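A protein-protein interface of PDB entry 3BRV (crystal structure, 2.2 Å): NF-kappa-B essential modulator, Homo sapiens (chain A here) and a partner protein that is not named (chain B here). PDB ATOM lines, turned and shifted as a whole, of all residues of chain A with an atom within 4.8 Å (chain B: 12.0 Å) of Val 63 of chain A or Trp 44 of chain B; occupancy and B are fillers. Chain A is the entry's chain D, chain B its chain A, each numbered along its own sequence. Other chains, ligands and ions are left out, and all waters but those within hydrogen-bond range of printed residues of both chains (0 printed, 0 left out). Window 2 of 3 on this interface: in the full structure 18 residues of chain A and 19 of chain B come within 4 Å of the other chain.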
ATOM      1  N   PHE A  56      -9.666   1.497   6.587  1.00  0.00           N
ATOM      2  CA  PHE A  56      -9.732   0.389   5.642  1.00  0.00           C
ATOM      3  C   PHE A  56     -10.897   0.564   4.663  1.00  0.00           C
ATOM      4  O   PHE A  56     -10.708   0.486   3.514  1.00  0.00           O
ATOM      5  CB  PHE A  56      -9.933  -0.954   6.389  1.00  0.00           C
ATOM      6  CG  PHE A  56     -10.211  -2.188   5.447  1.00  0.00           C
ATOM      7  CD1 PHE A  56      -9.165  -2.921   4.894  1.00  0.00           C
ATOM      8  CD2 PHE A  56     -11.530  -2.609   5.163  1.00  0.00           C
ATOM      9  CE1 PHE A  56      -9.380  -4.060   4.055  1.00  0.00           C
ATOM     10  CE2 PHE A  56     -11.762  -3.731   4.320  1.00  0.00           C
ATOM     11  CZ  PHE A  56     -10.673  -4.471   3.770  1.00  0.00           C
ATOM     12  N   ALA A  59     -10.356   3.572   2.463  1.00  0.00           N
ATOM     13  CA  ALA A  59      -9.265   3.349   1.476  1.00  0.00           C
ATOM     14  C   ALA A  59      -9.677   2.388   0.338  1.00  0.00           C
ATOM     15  O   ALA A  59      -9.284   2.617  -0.843  1.00  0.00           O
ATOM     16  CB  ALA A  59      -8.015   2.861   2.100  1.00  0.00           C
ATOM     17  N   ARG A  60     -10.414   1.312   0.685  1.00  0.00           N
ATOM     18  CA  ARG A  60     -10.986   0.377  -0.322  1.00  0.00           C
ATOM     19  C   ARG A  60     -11.876   1.147  -1.316  1.00  0.00           C
ATOM     20  O   ARG A  60     -11.726   0.977  -2.535  1.00  0.00           O
ATOM     21  CB  ARG A  60     -11.738  -0.829   0.292  1.00  0.00           C
ATOM     22  N   LYS A  61     -12.766   2.004  -0.806  1.00  0.00           N
ATOM     23  CA  LYS A  61     -13.680   2.826  -1.649  1.00  0.00           C
ATOM     24  C   LYS A  61     -12.993   3.884  -2.448  1.00  0.00           C
ATOM     25  O   LYS A  61     -13.348   4.120  -3.571  1.00  0.00           O
ATOM     26  CB  LYS A  61     -14.898   3.399  -0.858  1.00  0.00           C
ATOM     27  N   LEU A  62     -11.950   4.503  -1.921  1.00  0.00           N
ATOM     28  CA  LEU A  62     -11.180   5.442  -2.715  1.00  0.00           C
ATOM     29  C   LEU A  62     -10.415   4.717  -3.782  1.00  0.00           C
ATOM     30  O   LEU A  62     -10.255   5.196  -4.907  1.00  0.00           O
ATOM     31  CB  LEU A  62     -10.255   6.320  -1.886  1.00  0.00           C
ATOM     32  CG  LEU A  62      -9.273   7.250  -2.606  1.00  0.00           C
ATOM     33  CD1 LEU A  62     -10.205   8.263  -3.372  1.00  0.00           C
ATOM     34  CD2 LEU A  62      -8.290   8.021  -1.630  1.00  0.00           C
ATOM     35  N   VAL A  63      -9.962   3.542  -3.505  1.00  0.00           N
ATOM     36  CA  VAL A  63      -9.291   2.810  -4.620  1.00  0.00           C
ATOM     37  C   VAL A  63     -10.321   2.377  -5.675  1.00  0.00           C
ATOM     38  O   VAL A  63      -9.963   2.193  -6.861  1.00  0.00           O
ATOM     39  CB  VAL A  63      -8.502   1.575  -4.115  1.00  0.00           C
ATOM     40  CG1 VAL A  63      -8.267   0.530  -5.260  1.00  0.00           C
ATOM     41  CG2 VAL A  63      -7.168   2.002  -3.484  1.00  0.00           C
ATOM     42  N   GLU A  64     -11.579   2.199  -5.257  1.00  0.00           N
ATOM     43  CA  GLU A  64     -12.631   1.739  -6.161  1.00  0.00           C
ATOM     44  C   GLU A  64     -12.870   2.891  -7.127  1.00  0.00           C
ATOM     45  O   GLU A  64     -12.809   2.693  -8.344  1.00  0.00           O
ATOM     46  CB  GLU A  64     -13.934   1.285  -5.397  1.00  0.00           C
ATOM     47  CG  GLU A  64     -15.155   0.767  -6.310  1.00  0.00           C
ATOM     48  CD  GLU A  64     -16.504   0.460  -5.533  1.00  0.00           C
ATOM     49  OE1 GLU A  64     -16.518   0.641  -4.293  1.00  0.00           O
ATOM     50  OE2 GLU A  64     -17.531   0.001  -6.178  1.00  0.00           O
ATOM     51  N   ARG A  65     -13.073   4.096  -6.545  1.00  0.00           N
ATOM     52  CA  ARG A  65     -13.298   5.333  -7.224  1.00  0.00           C
ATOM     53  C   ARG A  65     -12.215   5.622  -8.289  1.00  0.00           C
ATOM     54  O   ARG A  65     -12.536   5.735  -9.492  1.00  0.00           O
ATOM     55  CB  ARG A  65     -13.331   6.447  -6.231  1.00  0.00           C
ATOM     56  CG  ARG A  65     -13.230   7.791  -6.945  1.00  0.00           C
ATOM     57  CD  ARG A  65     -13.440   9.020  -6.018  1.00  0.00           C
ATOM     58  NE  ARG A  65     -14.723   8.993  -5.349  1.00  0.00           N
ATOM     59  CZ  ARG A  65     -15.163   9.911  -4.477  1.00  0.00           C
ATOM     60  NH1 ARG A  65     -14.386  10.957  -4.159  1.00  0.00           N
ATOM     61  NH2 ARG A  65     -16.369   9.771  -3.888  1.00  0.00           N
ATOM     62  N   LEU A  66     -10.939   5.620  -7.853  1.00  0.00           N
ATOM     63  CA  LEU A  66      -9.795   5.931  -8.699  1.00  0.00           C
ATOM     64  C   LEU A  66      -9.542   4.944  -9.827  1.00  0.00           C
ATOM     65  O   LEU A  66      -9.151   5.366 -10.903  1.00  0.00           O
ATOM     66  CB  LEU A  66      -8.529   6.056  -7.843  1.00  0.00           C
ATOM     67  CG  LEU A  66      -8.109   7.368  -7.240  1.00  0.00           C
ATOM     68  CD1 LEU A  66      -8.961   8.541  -7.617  1.00  0.00           C
ATOM     69  CD2 LEU A  66      -7.939   7.251  -5.733  1.00  0.00           C
ATOM     70  N   GLY A  67      -9.746   3.653  -9.572  1.00  0.00           N
ATOM     71  CA  GLY A  67      -9.602   2.576 -10.581  1.00  0.00           C
ATOM     72  C   GLY A  67     -10.587   2.667 -11.746  1.00  0.00           C
ATOM     73  O   GLY A  67     -10.313   2.173 -12.853  1.00  0.00           O
ATOM     74  N   SER B  36      -8.141 -10.539  13.697  1.00  0.00           N
ATOM     75  CA  SER B  36      -7.056  -9.812  12.977  1.00  0.00           C
ATOM     76  C   SER B  36      -7.484  -9.221  11.633  1.00  0.00           C
ATOM     77  O   SER B  36      -8.380  -9.765  10.896  1.00  0.00           O
ATOM     78  CB  SER B  36      -5.793 -10.692  12.879  1.00  0.00           C
ATOM     79  OG  SER B  36      -4.898 -10.254  11.856  1.00  0.00           O
ATOM     80  N   PHE B  37      -6.829  -8.122  11.282  1.00  0.00           N
ATOM     81  CA  PHE B  37      -7.049  -7.470   9.998  1.00  0.00           C
ATOM     82  C   PHE B  37      -6.524  -8.272   8.828  1.00  0.00           C
ATOM     83  O   PHE B  37      -6.880  -8.018   7.676  1.00  0.00           O
ATOM     84  CB  PHE B  37      -6.448  -6.075  10.038  1.00  0.00           C
ATOM     85  CG  PHE B  37      -7.303  -5.042  10.798  1.00  0.00           C
ATOM     86  CD1 PHE B  37      -7.218  -4.901  12.156  1.00  0.00           C
ATOM     87  CD2 PHE B  37      -8.164  -4.178  10.105  1.00  0.00           C
ATOM     88  CE1 PHE B  37      -8.009  -3.926  12.848  1.00  0.00           C
ATOM     89  CE2 PHE B  37      -8.943  -3.193  10.775  1.00  0.00           C
ATOM     90  CZ  PHE B  37      -8.868  -3.092  12.141  1.00  0.00           C
ATOM     91  N   THR B  38      -5.686  -9.269   9.141  1.00  0.00           N
ATOM     92  CA  THR B  38      -5.200 -10.291   8.200  1.00  0.00           C
ATOM     93  C   THR B  38      -6.364 -11.053   7.624  1.00  0.00           C
ATOM     94  O   THR B  38      -6.220 -11.636   6.584  1.00  0.00           O
ATOM     95  CB  THR B  38      -4.122 -11.294   8.841  1.00  0.00           C
ATOM     96  OG1 THR B  38      -4.708 -12.017   9.940  1.00  0.00           O
ATOM     97  CG2 THR B  38      -2.972 -10.538   9.371  1.00  0.00           C
ATOM     98  N   ALA B  39      -7.504 -11.011   8.295  1.00  0.00           N
ATOM     99  CA  ALA B  39      -8.756 -11.676   7.848  1.00  0.00           C
ATOM    100  C   ALA B  39      -9.577 -10.970   6.789  1.00  0.00           C
ATOM    101  O   ALA B  39     -10.444 -11.559   6.120  1.00  0.00           O
ATOM    102  CB  ALA B  39      -9.688 -11.885   9.088  1.00  0.00           C
ATOM    103  N   LEU B  40      -9.429  -9.679   6.735  1.00  0.00           N
ATOM    104  CA  LEU B  40     -10.075  -8.865   5.756  1.00  0.00           C
ATOM    105  C   LEU B  40      -9.505  -9.265   4.415  1.00  0.00           C
ATOM    106  O   LEU B  40      -8.428  -9.841   4.316  1.00  0.00           O
ATOM    107  CB  LEU B  40      -9.822  -7.367   6.062  1.00  0.00           C
ATOM    108  CG  LEU B  40     -10.397  -6.878   7.416  1.00  0.00           C
ATOM    109  CD1 LEU B  40      -9.967  -5.484   7.799  1.00  0.00           C
ATOM    110  CD2 LEU B  40     -11.896  -6.984   7.455  1.00  0.00           C
ATOM    111  N   ASP B  41     -10.278  -9.006   3.370  1.00  0.00           N
ATOM    112  CA  ASP B  41      -9.838  -9.155   2.034  1.00  0.00           C
ATOM    113  C   ASP B  41      -9.035  -7.934   1.612  1.00  0.00           C
ATOM    114  O   ASP B  41      -9.590  -6.838   1.588  1.00  0.00           O
ATOM    115  CB  ASP B  41     -11.076  -9.231   1.147  1.00  0.00           C
ATOM    116  CG  ASP B  41     -10.719  -9.544  -0.263  1.00  0.00           C
ATOM    117  OD1 ASP B  41     -10.218 -10.652  -0.459  1.00  0.00           O
ATOM    118  OD2 ASP B  41     -10.868  -8.697  -1.162  1.00  0.00           O
ATOM    119  N   TRP B  42      -7.747  -8.097   1.288  1.00  0.00           N
ATOM    120  CA  TRP B  42      -6.906  -6.956   0.901  1.00  0.00           C
ATOM    121  C   TRP B  42      -6.545  -7.020  -0.605  1.00  0.00           C
ATOM    122  O   TRP B  42      -5.705  -6.312  -1.097  1.00  0.00           O
ATOM    123  CB  TRP B  42      -5.625  -6.955   1.742  1.00  0.00           C
ATOM    124  CG  TRP B  42      -5.815  -6.628   3.173  1.00  0.00           C
ATOM    125  CD1 TRP B  42      -5.970  -7.514   4.227  1.00  0.00           C
ATOM    126  CD2 TRP B  42      -5.880  -5.324   3.726  1.00  0.00           C
ATOM    127  NE1 TRP B  42      -6.155  -6.813   5.433  1.00  0.00           N
ATOM    128  CE2 TRP B  42      -6.029  -5.471   5.156  1.00  0.00           C
ATOM    129  CE3 TRP B  42      -5.721  -4.028   3.182  1.00  0.00           C
ATOM    130  CZ2 TRP B  42      -6.076  -4.361   6.025  1.00  0.00           C
ATOM    131  CZ3 TRP B  42      -5.796  -2.920   4.053  1.00  0.00           C
ATOM    132  CH2 TRP B  42      -5.962  -3.104   5.455  1.00  0.00           C
ATOM    133  N   SER B  43      -7.231  -7.844  -1.345  1.00  0.00           N
ATOM    134  CA  SER B  43      -6.884  -8.069  -2.763  1.00  0.00           C
ATOM    135  C   SER B  43      -7.226  -6.855  -3.662  1.00  0.00           C
ATOM    136  O   SER B  43      -6.758  -6.747  -4.786  1.00  0.00           O
ATOM    137  CB  SER B  43      -7.600  -9.319  -3.238  1.00  0.00           C
ATOM    138  OG  SER B  43      -9.011  -9.120  -3.306  1.00  0.00           O
ATOM    139  N   TRP B  44      -8.012  -5.905  -3.155  1.00  0.00           N
ATOM    140  CA  TRP B  44      -8.240  -4.647  -3.908  1.00  0.00           C
ATOM    141  C   TRP B  44      -6.972  -3.762  -3.961  1.00  0.00           C
ATOM    142  O   TRP B  44      -6.947  -2.772  -4.678  1.00  0.00           O
ATOM    143  CB  TRP B  44      -9.398  -3.884  -3.285  1.00  0.00           C
ATOM    144  CG  TRP B  44      -9.189  -3.668  -1.807  1.00  0.00           C
ATOM    145  CD1 TRP B  44      -9.563  -4.506  -0.796  1.00  0.00           C
ATOM    146  CD2 TRP B  44      -8.453  -2.595  -1.193  1.00  0.00           C
ATOM    147  NE1 TRP B  44      -9.127  -4.013   0.431  1.00  0.00           N
ATOM    148  CE2 TRP B  44      -8.448  -2.842   0.223  1.00  0.00           C
ATOM    149  CE3 TRP B  44      -7.801  -1.453  -1.689  1.00  0.00           C
ATOM    150  CZ2 TRP B  44      -7.879  -1.962   1.143  1.00  0.00           C
ATOM    151  CZ3 TRP B  44      -7.222  -0.544  -0.736  1.00  0.00           C
ATOM    152  CH2 TRP B  44      -7.280  -0.816   0.658  1.00  0.00           C
ATOM    153  N   LEU B  45      -5.936  -4.116  -3.193  1.00  0.00           N
ATOM    154  CA  LEU B  45      -4.602  -3.513  -3.327  1.00  0.00           C
ATOM    155  C   LEU B  45      -3.929  -3.976  -4.603  1.00  0.00           C
ATOM    156  O   LEU B  45      -2.943  -3.381  -5.033  1.00  0.00           O
ATOM    157  CB  LEU B  45      -3.710  -3.848  -2.137  1.00  0.00           C
ATOM    158  CG  LEU B  45      -4.305  -3.335  -0.838  1.00  0.00           C
ATOM    159  CD1 LEU B  45      -3.603  -4.035   0.306  1.00  0.00           C
ATOM    160  CD2 LEU B  45      -4.122  -1.870  -0.760  1.00  0.00           C
ATOM    161  N   GLN B  46      -4.433  -5.113  -5.117  1.00  0.00           N
ATOM    162  CA  GLN B  46      -4.460  -5.619  -6.561  1.00  0.00           C
ATOM    163  C   GLN B  46      -4.180  -7.115  -6.586  1.00  0.00           C
ATOM    164  O   GLN B  46      -3.440  -7.609  -5.718  1.00  0.00           O
ATOM    165  CB  GLN B  46      -3.544  -4.874  -7.552  1.00  0.00           C
ATOM    166  CG  GLN B  46      -4.220  -4.509  -8.908  1.00  0.00           C
ATOM    167  CD  GLN B  46      -5.339  -3.416  -8.791  1.00  0.00           C
ATOM    168  OE1 GLN B  46      -5.347  -2.384  -9.526  1.00  0.00           O
ATOM    169  NE2 GLN B  46      -6.292  -3.659  -7.885  1.00  0.00           N
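The backbone carbonyl oxygen (O) of Asp 41 of chain B sits at hydrogen-bond distance from the indole nitrogen (NE1) of Trp 44 of chain B, at 3.1 Å.
OD2 of Asp 41 of chain B lies within hydrogen-bond range of OG of Ser 43 of chain B, 2.9 Å away.
NE1 of Trp 42 of chain B sits at hydrogen-bond distance from O of Phe 37 of chain B.
O of Trp 44 of chain B sits at hydrogen-bond distance from NE2 of Gln 46 of chain B (3.4 Å).
Of chain B, only Leu 40 (3.8 Å), Asp 41 (3.4 Å), Trp 42 (3.3 Å) and Trp 44 (3.6 Å) come within 4 Å of Phe 56 of chain A.
Ala 59 of chain A touches just one residue of chain B: Trp 44 (3.8 Å).
Of chain B, only Trp 44 comes within 4 Å of Arg 60 of chain A.
No residue of chain B comes within 4 Å of Lys 61 of chain A.
No residue of chain B comes within 4 Å of Leu 62 of chain A.
Of chain B, only Trp 44 comes within 4 Å of Val 63 of chain A.
Arg 65 of chain A touches none of the printed residues of chain B.
No residue of chain B comes within 4 Å of Leu 66 of chain A.
Gly 67 of chain A touches none of the printed residues of chain B.
Of the printed residues of chain A, Leu 40 of chain B touches Phe 56 (3.8 Å).
Of the printed residues of chain A, Trp 42 of chain B touches Phe 56.
Trp 44 of chain B touches four residues of chain A.
The nearest printed residue of chain A that does not touch Trp 44 of chain B is Lys 61 of chain A (6.1 Å).
Of the 10 printed residues of chain A, 4 touch a printed residue of chain B.
Hydrophobic or aromatic side chains of chain A that line the printed part of chain B: Phe 56 and Val 63.
Of the 11 printed residues of chain B, 4 touch a printed residue of chain A.
Hydrophobic or aromatic side chains of chain B within 4 Å of the printed part of chain A: Leu 40, Trp 42 and Trp 44.
Among the printed residues, no Asp or Glu carboxylate lies within 4 Å of a Lys or Arg side-chain nitrogen of the other chain.
CZ of Phe 56 of chain A touches CB of Leu 40 of chain B (3.8 Å).
Phe 56 of chain A touches Asp 41 of chain B (CZ to O, 3.4 Å).
CH2 of Trp 42 of chain B touches CD1 of Phe 56 of chain A, at 3.3 Å.
Trp 44 of chain B touches Phe 56 of chain A.
O of Ala 59 of chain A touches CZ3 of Trp 44 of chain B, at 3.8 Å.
Trp 44 of chain B touches Arg 60 of chain A.
O of Trp 44 of chain B touches CG1 of Val 63 of chain A, 3.6 Å away.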
